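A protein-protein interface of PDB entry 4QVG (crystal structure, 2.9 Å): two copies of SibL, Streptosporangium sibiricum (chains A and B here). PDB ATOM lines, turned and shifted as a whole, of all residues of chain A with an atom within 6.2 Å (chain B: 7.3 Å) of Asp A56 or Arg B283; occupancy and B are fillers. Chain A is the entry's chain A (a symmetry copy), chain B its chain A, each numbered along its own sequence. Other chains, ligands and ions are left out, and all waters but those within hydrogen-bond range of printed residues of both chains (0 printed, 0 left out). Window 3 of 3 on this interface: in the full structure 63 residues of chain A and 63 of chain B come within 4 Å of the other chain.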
ATOM      1  N   ALA A  41       1.022  -4.852 -32.489  1.00  0.00           N
ATOM      2  CA  ALA A  41       2.432  -4.937 -32.185  1.00  0.00           C
ATOM      3  C   ALA A  41       3.185  -3.889 -33.001  1.00  0.00           C
ATOM      4  O   ALA A  41       4.026  -3.160 -32.471  1.00  0.00           O
ATOM      5  CB  ALA A  41       2.945  -6.303 -32.474  1.00  0.00           C
ATOM      6  N   GLU A  42       2.862  -3.792 -34.288  1.00  0.00           N
ATOM      7  CA  GLU A  42       3.568  -2.876 -35.174  1.00  0.00           C
ATOM      8  C   GLU A  42       3.359  -1.399 -34.776  1.00  0.00           C
ATOM      9  O   GLU A  42       4.298  -0.591 -34.808  1.00  0.00           O
ATOM     10  CB  GLU A  42       3.090  -3.106 -36.585  1.00  0.00           C
ATOM     11  CG  GLU A  42       4.008  -2.593 -37.673  1.00  0.00           C
ATOM     12  CD  GLU A  42       3.587  -3.139 -39.028  1.00  0.00           C
ATOM     13  OE1 GLU A  42       2.599  -2.617 -39.584  1.00  0.00           O
ATOM     14  OE2 GLU A  42       4.174  -4.148 -39.485  1.00  0.00           O
ATOM     15  N   PRO A  51      12.901  -1.577 -32.397  1.00  0.00           N
ATOM     16  CA  PRO A  51      12.978  -2.633 -33.406  1.00  0.00           C
ATOM     17  C   PRO A  51      11.812  -3.556 -33.208  1.00  0.00           C
ATOM     18  O   PRO A  51      11.467  -3.818 -32.077  1.00  0.00           O
ATOM     19  CB  PRO A  51      14.283  -3.347 -33.057  1.00  0.00           C
ATOM     20  CG  PRO A  51      15.131  -2.263 -32.474  1.00  0.00           C
ATOM     21  CD  PRO A  51      14.177  -1.375 -31.698  1.00  0.00           C
ATOM     22  N   ARG A  52      11.230  -4.065 -34.272  1.00  0.00           N
ATOM     23  CA  ARG A  52      10.049  -4.907 -34.163  1.00  0.00           C
ATOM     24  C   ARG A  52      10.363  -6.133 -33.304  1.00  0.00           C
ATOM     25  O   ARG A  52       9.526  -6.578 -32.516  1.00  0.00           O
ATOM     26  CB  ARG A  52       9.565  -5.341 -35.550  1.00  0.00           C
ATOM     27  CG  ARG A  52       8.418  -6.324 -35.523  1.00  0.00           C
ATOM     28  CD  ARG A  52       7.250  -5.760 -34.742  1.00  0.00           C
ATOM     29  NE  ARG A  52       6.268  -6.814 -34.505  1.00  0.00           N
ATOM     30  CZ  ARG A  52       5.247  -7.096 -35.312  1.00  0.00           C
ATOM     31  NH1 ARG A  52       5.043  -6.395 -36.429  1.00  0.00           N
ATOM     32  NH2 ARG A  52       4.426  -8.087 -34.992  1.00  0.00           N
ATOM     33  N   ARG A  53      11.569  -6.676 -33.465  1.00  0.00           N
ATOM     34  CA  ARG A  53      11.974  -7.838 -32.687  1.00  0.00           C
ATOM     35  C   ARG A  53      11.879  -7.500 -31.190  1.00  0.00           C
ATOM     36  O   ARG A  53      11.251  -8.218 -30.384  1.00  0.00           O
ATOM     37  CB  ARG A  53      13.396  -8.206 -33.045  1.00  0.00           C
ATOM     38  CG  ARG A  53      13.750  -9.611 -32.860  1.00  0.00           C
ATOM     39  CD  ARG A  53      15.224  -9.776 -33.100  1.00  0.00           C
ATOM     40  NE  ARG A  53      15.957  -9.619 -31.844  1.00  0.00           N
ATOM     41  CZ  ARG A  53      16.247 -10.623 -31.013  1.00  0.00           C
ATOM     42  NH1 ARG A  53      15.872 -11.879 -31.312  1.00  0.00           N
ATOM     43  NH2 ARG A  53      16.926 -10.364 -29.890  1.00  0.00           N
ATOM     44  N   SER A  54      12.425  -6.342 -30.850  1.00  0.00           N
ATOM     45  CA  SER A  54      12.400  -5.880 -29.491  1.00  0.00           C
ATOM     46  C   SER A  54      10.976  -5.730 -28.997  1.00  0.00           C
ATOM     47  O   SER A  54      10.661  -6.191 -27.896  1.00  0.00           O
ATOM     48  CB  SER A  54      13.184  -4.586 -29.359  1.00  0.00           C
ATOM     49  OG  SER A  54      14.539  -4.860 -29.657  1.00  0.00           O
ATOM     50  N   ALA A  55      10.107  -5.113 -29.795  1.00  0.00           N
ATOM     51  CA  ALA A  55       8.726  -4.938 -29.338  1.00  0.00           C
ATOM     52  C   ALA A  55       8.003  -6.274 -29.170  1.00  0.00           C
ATOM     53  O   ALA A  55       7.241  -6.442 -28.223  1.00  0.00           O
ATOM     54  CB  ALA A  55       7.953  -4.047 -30.262  1.00  0.00           C
ATOM     55  N   ASP A  56       8.263  -7.235 -30.050  1.00  0.00           N
ATOM     56  CA  ASP A  56       7.588  -8.514 -29.928  1.00  0.00           C
ATOM     57  C   ASP A  56       7.951  -9.222 -28.617  1.00  0.00           C
ATOM     58  O   ASP A  56       7.078  -9.729 -27.903  1.00  0.00           O
ATOM     59  CB  ASP A  56       7.923  -9.408 -31.124  1.00  0.00           C
ATOM     60  CG  ASP A  56       7.148  -9.021 -32.388  1.00  0.00           C
ATOM     61  OD1 ASP A  56       6.101  -8.346 -32.258  1.00  0.00           O
ATOM     62  OD2 ASP A  56       7.551  -9.436 -33.507  1.00  0.00           O
ATOM     63  N   ILE A  57       9.236  -9.172 -28.283  1.00  0.00           N
ATOM     64  CA  ILE A  57       9.791  -9.727 -27.052  1.00  0.00           C
ATOM     65  C   ILE A  57       9.211  -9.059 -25.804  1.00  0.00           C
ATOM     66  O   ILE A  57       8.771  -9.734 -24.861  1.00  0.00           O
ATOM     67  CB  ILE A  57      11.324  -9.602 -27.063  1.00  0.00           C
ATOM     68  CG1 ILE A  57      11.917 -10.637 -28.020  1.00  0.00           C
ATOM     69  CG2 ILE A  57      11.899  -9.756 -25.671  1.00  0.00           C
ATOM     70  CD1 ILE A  57      13.295 -10.281 -28.518  1.00  0.00           C
ATOM     71  N   LEU A  58       9.246  -7.733 -25.775  1.00  0.00           N
ATOM     72  CA  LEU A  58       8.657  -7.001 -24.668  1.00  0.00           C
ATOM     73  C   LEU A  58       7.179  -7.342 -24.500  1.00  0.00           C
ATOM     74  O   LEU A  58       6.695  -7.472 -23.385  1.00  0.00           O
ATOM     75  CB  LEU A  58       8.826  -5.494 -24.845  1.00  0.00           C
ATOM     76  CG  LEU A  58       8.091  -4.639 -23.811  1.00  0.00           C
ATOM     77  CD1 LEU A  58       8.635  -4.886 -22.421  1.00  0.00           C
ATOM     78  CD2 LEU A  58       8.105  -3.153 -24.158  1.00  0.00           C
ATOM     79  N   LEU A  59       6.461  -7.491 -25.608  1.00  0.00           N
ATOM     80  CA  LEU A  59       5.025  -7.689 -25.525  1.00  0.00           C
ATOM     81  C   LEU A  59       4.717  -9.096 -25.062  1.00  0.00           C
ATOM     82  O   LEU A  59       3.697  -9.311 -24.414  1.00  0.00           O
ATOM     83  CB  LEU A  59       4.324  -7.392 -26.854  1.00  0.00           C
ATOM     84  CG  LEU A  59       4.159  -5.912 -27.225  1.00  0.00           C
ATOM     85  CD1 LEU A  59       3.595  -5.739 -28.655  1.00  0.00           C
ATOM     86  CD2 LEU A  59       3.337  -5.107 -26.187  1.00  0.00           C
ATOM     87  N   LEU A  60       5.585 -10.048 -25.395  1.00  0.00           N
ATOM     88  CA  LEU A  60       5.413 -11.419 -24.923  1.00  0.00           C
ATOM     89  C   LEU A  60       5.680 -11.470 -23.406  1.00  0.00           C
ATOM     90  O   LEU A  60       5.000 -12.175 -22.650  1.00  0.00           O
ATOM     91  CB  LEU A  60       6.368 -12.357 -25.662  1.00  0.00           C
ATOM     92  CG  LEU A  60       6.295 -13.813 -25.217  1.00  0.00           C
ATOM     93  CD1 LEU A  60       4.861 -14.300 -25.359  1.00  0.00           C
ATOM     94  CD2 LEU A  60       7.221 -14.674 -26.045  1.00  0.00           C
ATOM     95  N   GLY A  61       6.702 -10.734 -22.978  1.00  0.00           N
ATOM     96  CA  GLY A  61       7.010 -10.620 -21.576  1.00  0.00           C
ATOM     97  C   GLY A  61       5.786 -10.091 -20.856  1.00  0.00           C
ATOM     98  O   GLY A  61       5.225 -10.747 -19.965  1.00  0.00           O
ATOM     99  N   THR A  63       2.789  -9.800 -21.659  1.00  0.00           N
ATOM    100  CA  THR A  63       1.480 -10.415 -21.842  1.00  0.00           C
ATOM    101  C   THR A  63       1.407 -11.714 -21.057  1.00  0.00           C
ATOM    102  O   THR A  63       0.376 -12.033 -20.462  1.00  0.00           O
ATOM    103  CB  THR A  63       1.158 -10.627 -23.350  1.00  0.00           C
ATOM    104  OG1 THR A  63       1.083  -9.342 -23.975  1.00  0.00           O
ATOM    105  CG2 THR A  63      -0.140 -11.360 -23.557  1.00  0.00           C
ATOM    106  N   ALA A  64       2.508 -12.447 -21.045  1.00  0.00           N
ATOM    107  CA  ALA A  64       2.614 -13.650 -20.244  1.00  0.00           C
ATOM    108  C   ALA A  64       2.443 -13.382 -18.734  1.00  0.00           C
ATOM    109  O   ALA A  64       1.956 -14.250 -17.993  1.00  0.00           O
ATOM    110  CB  ALA A  64       3.947 -14.322 -20.513  1.00  0.00           C
ATOM    111  N   VAL A  70      -3.615  -9.494 -25.114  1.00  0.00           N
ATOM    112  CA  VAL A  70      -3.676  -9.370 -26.566  1.00  0.00           C
ATOM    113  C   VAL A  70      -4.934 -10.027 -27.110  1.00  0.00           C
ATOM    114  O   VAL A  70      -5.214 -11.202 -26.850  1.00  0.00           O
ATOM    115  CB  VAL A  70      -2.423  -9.946 -27.287  1.00  0.00           C
ATOM    116  CG1 VAL A  70      -2.202 -11.412 -26.929  1.00  0.00           C
ATOM    117  CG2 VAL A  70      -2.577  -9.797 -28.808  1.00  0.00           C
ATOM    118  N   TYR A  75      -3.227  -4.854 -28.457  1.00  0.00           N
ATOM    119  CA  TYR A  75      -2.765  -4.965 -27.091  1.00  0.00           C
ATOM    120  C   TYR A  75      -3.391  -3.943 -26.172  1.00  0.00           C
ATOM    121  O   TYR A  75      -3.367  -2.743 -26.449  1.00  0.00           O
ATOM    122  CB  TYR A  75      -1.242  -4.823 -27.064  1.00  0.00           C
ATOM    123  CG  TYR A  75      -0.523  -5.996 -27.690  1.00  0.00           C
ATOM    124  CD1 TYR A  75      -0.308  -6.060 -29.065  1.00  0.00           C
ATOM    125  CD2 TYR A  75      -0.060  -7.050 -26.902  1.00  0.00           C
ATOM    126  CE1 TYR A  75       0.350  -7.150 -29.635  1.00  0.00           C
ATOM    127  CE2 TYR A  75       0.598  -8.145 -27.469  1.00  0.00           C
ATOM    128  CZ  TYR A  75       0.797  -8.186 -28.834  1.00  0.00           C
ATOM    129  OH  TYR A  75       1.440  -9.265 -29.391  1.00  0.00           O
ATOM    130  N   TYR B 111      18.194  -4.662 -19.962  1.00  0.00           N
ATOM    131  CA  TYR B 111      17.115  -5.081 -20.873  1.00  0.00           C
ATOM    132  C   TYR B 111      16.556  -3.903 -21.660  1.00  0.00           C
ATOM    133  O   TYR B 111      16.371  -3.984 -22.861  1.00  0.00           O
ATOM    134  CB  TYR B 111      16.006  -5.688 -20.037  1.00  0.00           C
ATOM    135  CG  TYR B 111      14.853  -6.341 -20.736  1.00  0.00           C
ATOM    136  CD1 TYR B 111      15.045  -7.343 -21.676  1.00  0.00           C
ATOM    137  CD2 TYR B 111      13.543  -5.998 -20.386  1.00  0.00           C
ATOM    138  CE1 TYR B 111      13.954  -7.981 -22.277  1.00  0.00           C
ATOM    139  CE2 TYR B 111      12.441  -6.616 -20.978  1.00  0.00           C
ATOM    140  CZ  TYR B 111      12.652  -7.614 -21.926  1.00  0.00           C
ATOM    141  OH  TYR B 111      11.559  -8.228 -22.500  1.00  0.00           O
ATOM    142  N   LEU B 115      16.682  -3.630 -25.650  1.00  0.00           N
ATOM    143  CA  LEU B 115      15.544  -3.650 -26.526  1.00  0.00           C
ATOM    144  C   LEU B 115      15.675  -2.452 -27.479  1.00  0.00           C
ATOM    145  O   LEU B 115      15.521  -2.595 -28.687  1.00  0.00           O
ATOM    146  CB  LEU B 115      14.254  -3.563 -25.729  1.00  0.00           C
ATOM    147  CG  LEU B 115      13.830  -4.694 -24.784  1.00  0.00           C
ATOM    148  CD1 LEU B 115      12.560  -4.251 -24.045  1.00  0.00           C
ATOM    149  CD2 LEU B 115      13.590  -5.995 -25.475  1.00  0.00           C
ATOM    150  N   THR B 279       7.469 -20.567 -28.681  1.00  0.00           N
ATOM    151  CA  THR B 279       6.469 -19.611 -28.226  1.00  0.00           C
ATOM    152  C   THR B 279       5.082 -20.091 -28.649  1.00  0.00           C
ATOM    153  O   THR B 279       4.926 -20.731 -29.688  1.00  0.00           O
ATOM    154  CB  THR B 279       6.733 -18.223 -28.841  1.00  0.00           C
ATOM    155  OG1 THR B 279       8.051 -17.799 -28.480  1.00  0.00           O
ATOM    156  CG2 THR B 279       5.748 -17.206 -28.332  1.00  0.00           C
ATOM    157  N   ASP B 280       4.077 -19.830 -27.821  1.00  0.00           N
ATOM    158  CA  ASP B 280       2.719 -20.173 -28.201  1.00  0.00           C
ATOM    159  C   ASP B 280       2.289 -19.341 -29.406  1.00  0.00           C
ATOM    160  O   ASP B 280       2.716 -18.190 -29.563  1.00  0.00           O
ATOM    161  CB  ASP B 280       1.772 -19.967 -27.023  1.00  0.00           C
ATOM    162  CG  ASP B 280       1.949 -21.020 -25.953  1.00  0.00           C
ATOM    163  OD1 ASP B 280       2.327 -22.168 -26.314  1.00  0.00           O
ATOM    164  OD2 ASP B 280       1.726 -20.686 -24.759  1.00  0.00           O
ATOM    165  N   ASP B 281       1.423 -19.912 -30.234  1.00  0.00           N
ATOM    166  CA  ASP B 281       1.000 -19.244 -31.458  1.00  0.00           C
ATOM    167  C   ASP B 281       0.314 -17.915 -31.170  1.00  0.00           C
ATOM    168  O   ASP B 281       0.403 -16.976 -31.971  1.00  0.00           O
ATOM    169  CB  ASP B 281       0.070 -20.130 -32.287  1.00  0.00           C
ATOM    170  CG  ASP B 281       0.783 -21.337 -32.881  1.00  0.00           C
ATOM    171  OD1 ASP B 281       2.037 -21.326 -32.953  1.00  0.00           O
ATOM    172  OD2 ASP B 281       0.087 -22.304 -33.268  1.00  0.00           O
ATOM    173  N   ASP B 282      -0.349 -17.814 -30.024  1.00  0.00           N
ATOM    174  CA  ASP B 282      -1.083 -16.594 -29.755  1.00  0.00           C
ATOM    175  C   ASP B 282      -0.210 -15.577 -29.075  1.00  0.00           C
ATOM    176  O   ASP B 282      -0.674 -14.486 -28.748  1.00  0.00           O
ATOM    177  CB  ASP B 282      -2.339 -16.853 -28.938  1.00  0.00           C
ATOM    178  CG  ASP B 282      -2.038 -17.435 -27.566  1.00  0.00           C
ATOM    179  OD1 ASP B 282      -0.840 -17.485 -27.167  1.00  0.00           O
ATOM    180  OD2 ASP B 282      -3.011 -17.842 -26.882  1.00  0.00           O
ATOM    181  N   ARG B 283       1.062 -15.934 -28.914  1.00  0.00           N
ATOM    182  CA  ARG B 283       2.073 -15.055 -28.325  1.00  0.00           C
ATOM    183  C   ARG B 283       1.724 -14.548 -26.921  1.00  0.00           C
ATOM    184  O   ARG B 283       2.058 -13.408 -26.586  1.00  0.00           O
ATOM    185  CB  ARG B 283       2.336 -13.871 -29.250  1.00  0.00           C
ATOM    186  CG  ARG B 283       2.709 -14.270 -30.658  1.00  0.00           C
ATOM    187  CD  ARG B 283       3.026 -13.054 -31.477  1.00  0.00           C
ATOM    188  NE  ARG B 283       4.455 -12.895 -31.588  1.00  0.00           N
ATOM    189  CZ  ARG B 283       5.174 -13.259 -32.633  1.00  0.00           C
ATOM    190  NH1 ARG B 283       4.580 -13.752 -33.692  1.00  0.00           N
ATOM    191  NH2 ARG B 283       6.484 -13.077 -32.630  1.00  0.00           N
ATOM    192  N   THR B 284       1.049 -15.385 -26.125  1.00  0.00           N
ATOM    193  CA  THR B 284       0.669 -15.056 -24.747  1.00  0.00           C
ATOM    194  C   THR B 284       1.520 -15.806 -23.754  1.00  0.00           C
ATOM    195  O   THR B 284       1.328 -15.664 -22.532  1.00  0.00           O
ATOM    196  CB  THR B 284      -0.773 -15.472 -24.437  1.00  0.00           C
ATOM    197  OG1 THR B 284      -0.926 -16.881 -24.692  1.00  0.00           O
ATOM    198  CG2 THR B 284      -1.760 -14.670 -25.263  1.00  0.00           C
ATOM    199  N   GLY B 285       2.451 -16.607 -24.275  1.00  0.00           N
ATOM    200  CA  GLY B 285       3.302 -17.438 -23.449  1.00  0.00           C
ATOM    201  C   GLY B 285       4.095 -18.447 -24.243  1.00  0.00           C
ATOM    202  O   GLY B 285       4.271 -18.293 -25.439  1.00  0.00           O
ATOM    203  N   PRO B 286       4.630 -19.474 -23.575  1.00  0.00           N
ATOM    204  CA  PRO B 286       4.523 -19.757 -22.149  1.00  0.00           C
ATOM    205  C   PRO B 286       5.443 -18.834 -21.335  1.00  0.00           C
ATOM    206  O   PRO B 286       6.427 -18.322 -21.857  1.00  0.00           O
ATOM    207  CB  PRO B 286       5.010 -21.200 -22.074  1.00  0.00           C
ATOM    208  CG  PRO B 286       6.013 -21.270 -23.082  1.00  0.00           C
ATOM    209  CD  PRO B 286       5.511 -20.451 -24.233  1.00  0.00           C
ATOM    210  N   ASN B 293      13.727 -14.690 -22.375  1.00  0.00           N
ATOM    211  CA  ASN B 293      14.260 -13.827 -23.418  1.00  0.00           C
ATOM    212  C   ASN B 293      15.131 -12.703 -22.888  1.00  0.00           C
ATOM    213  O   ASN B 293      15.950 -12.162 -23.619  1.00  0.00           O
ATOM    214  CB  ASN B 293      13.149 -13.262 -24.295  1.00  0.00           C
ATOM    215  CG  ASN B 293      12.634 -14.274 -25.277  1.00  0.00           C
ATOM    216  OD1 ASN B 293      13.373 -15.167 -25.734  1.00  0.00           O
ATOM    217  ND2 ASN B 293      11.342 -14.192 -25.560  1.00  0.00           N
ATOM    218  N   THR B 305      16.276 -16.484 -31.472  1.00  0.00           N
ATOM    219  CA  THR B 305      14.829 -16.327 -31.557  1.00  0.00           C
ATOM    220  C   THR B 305      14.060 -17.591 -31.218  1.00  0.00           C
ATOM    221  O   THR B 305      14.370 -18.668 -31.724  1.00  0.00           O
ATOM    222  CB  THR B 305      14.373 -15.781 -32.927  1.00  0.00           C
ATOM    223  OG1 THR B 305      15.035 -14.533 -33.161  1.00  0.00           O
ATOM    224  CG2 THR B 305      12.884 -15.501 -32.919  1.00  0.00           C
ATOM    225  N   ILE B 306      13.048 -17.454 -30.371  1.00  0.00           N
ATOM    226  CA  ILE B 306      12.127 -18.549 -30.125  1.00  0.00           C
ATOM    227  C   ILE B 306      10.910 -18.319 -31.030  1.00  0.00           C
ATOM    228  O   ILE B 306      10.067 -17.456 -30.789  1.00  0.00           O
ATOM    229  CB  ILE B 306      11.740 -18.659 -28.641  1.00  0.00           C
ATOM    230  CG1 ILE B 306      12.980 -18.940 -27.791  1.00  0.00           C
ATOM    231  CG2 ILE B 306      10.698 -19.733 -28.426  1.00  0.00           C
ATOM    232  CD1 ILE B 306      12.836 -18.440 -26.302  1.00  0.00           C
ATOM    233  N   HIS B 307      10.838 -19.101 -32.098  1.00  0.00           N
ATOM    234  CA  HIS B 307       9.763 -18.993 -33.069  1.00  0.00           C
ATOM    235  C   HIS B 307       8.503 -19.670 -32.551  1.00  0.00           C
ATOM    236  O   HIS B 307       8.583 -20.553 -31.703  1.00  0.00           O
ATOM    237  CB  HIS B 307      10.200 -19.684 -34.354  1.00  0.00           C
ATOM    238  CG  HIS B 307      11.605 -19.375 -34.764  1.00  0.00           C
ATOM    239  ND1 HIS B 307      11.939 -18.240 -35.474  1.00  0.00           N
ATOM    240  CD2 HIS B 307      12.766 -20.035 -34.538  1.00  0.00           C
ATOM    241  CE1 HIS B 307      13.243 -18.229 -35.691  1.00  0.00           C
ATOM    242  NE2 HIS B 307      13.768 -19.304 -35.129  1.00  0.00           N
ATOM    243  N   ARG B 308       7.330 -19.247 -33.013  1.00  0.00           N
ATOM    244  CA  ARG B 308       6.111 -19.939 -32.593  1.00  0.00           C
ATOM    245  C   ARG B 308       6.065 -21.299 -33.263  1.00  0.00           C
ATOM    246  O   ARG B 308       6.766 -21.524 -34.240  1.00  0.00           O
ATOM    247  CB  ARG B 308       4.868 -19.145 -32.974  1.00  0.00           C
ATOM    248  CG  ARG B 308       4.878 -17.744 -32.430  1.00  0.00           C
ATOM    249  CD  ARG B 308       4.390 -16.755 -33.447  1.00  0.00           C
ATOM    250  NE  ARG B 308       3.015 -17.045 -33.843  1.00  0.00           N
ATOM    251  CZ  ARG B 308       2.629 -17.227 -35.099  1.00  0.00           C
ATOM    252  NH1 ARG B 308       3.508 -17.134 -36.080  1.00  0.00           N
ATOM    253  NH2 ARG B 308       1.366 -17.491 -35.362  1.00  0.00           N
ATOM    254  N   ASP B 311       4.982 -20.786 -36.906  1.00  0.00           N
ATOM    255  CA  ASP B 311       6.090 -20.343 -37.750  1.00  0.00           C
ATOM    256  C   ASP B 311       6.864 -21.496 -38.304  1.00  0.00           C
ATOM    257  O   ASP B 311       7.171 -21.533 -39.493  1.00  0.00           O
ATOM    258  CB  ASP B 311       7.059 -19.468 -36.953  1.00  0.00           C
ATOM    259  CG  ASP B 311       6.502 -18.105 -36.657  1.00  0.00           C
ATOM    260  OD1 ASP B 311       5.682 -17.622 -37.482  1.00  0.00           O
ATOM    261  OD2 ASP B 311       6.836 -17.551 -35.573  1.00  0.00           O
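Among the printed residues, merely in contact across the chains: Leu A60 with Arg B283 (3.2 Å), Ala A64 with Thr B284 (3.3 Å), Leu A60 with Gly B285 (3.5 Å), Pro A51 with Leu B115 (3.5 Å), Ile A57 with Tyr B111 (3.5 Å), Val A70 with Thr B284 (3.7 Å), Leu A60 with Thr B279 (3.7 Å), Leu A58 with Tyr B111 (3.8 Å), Val A70 with Asp B282 (3.9 Å), Thr A63 with Thr B284 (3.97 Å) and Ile A57 with Asn B293 (3.97 Å).
Hydrophobic or aromatic side chains of chain B within 4 Å of the printed part of chain A: Tyr B111 and Leu B115.
Hydrophobic or aromatic side chains of chain A within 4 Å of the printed part of chain B: Pro A51, Ile A57, Leu A60, Ala A64 and Val A70.
Among the printed residues, Asp or Glu carboxylates within 4 Å of a Lys or Arg side-chain nitrogen of the other chain: Asp A56 with Arg B283 (3.9 Å).
The backbone carbonyl oxygen of Leu B115 is in hydrogen-bond range of the side-chain hydroxyl of Ser A54.
NH2 of Arg B283 lies within salt-bridge range of OD2 of Asp A56 (3.9 Å).
The side-chain hydroxyl (OG1) of Thr B305 is in hydrogen-bond range of the guanidinium group (NH1) of Arg A53 (3.3 Å).
The side-chain hydroxyl (OG1) of Thr B279 is in hydrogen-bond range of the backbone carbonyl oxygen (O) of Ile B306, at 3.1 Å.
The backbone NH (N) of Thr B279 lies within hydrogen-bond range of the backbone carbonyl oxygen (O) of His B307 (3.2 Å).
The backbone carbonyl oxygen (O) of Gly B285 sits at hydrogen-bond distance from the backbone NH (N) of Asp B280 (2.8 Å).
OG1 of Thr B284 lies within hydrogen-bond range of OD1 of Asp B282.
The side-chain carboxylate of Asp A56 is in salt-bridge range of the guanidinium group of Arg A52 (2.7 Å).
The backbone carbonyl oxygen of Leu A59 lies within hydrogen-bond range of the side-chain hydroxyl of Thr A63, 2.7 Å away.
Of chain B, only Arg B283 comes within 4 Å of Asp A56.
Of the printed residues of chain A, Thr B279 touches Leu A60.
Printed residues of chain B within 4 Å of Val A70: Asp B282 (3.9 Å) and Thr B284 (3.7 Å).
The nearest residue of chain A that does not touch Arg B283 is Thr A63 (4.3 Å).
No position is printed for both chains.
Of the 14 pairs that touch across the chains among the printed residues, none has its exchanged pair printed and touching as well.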
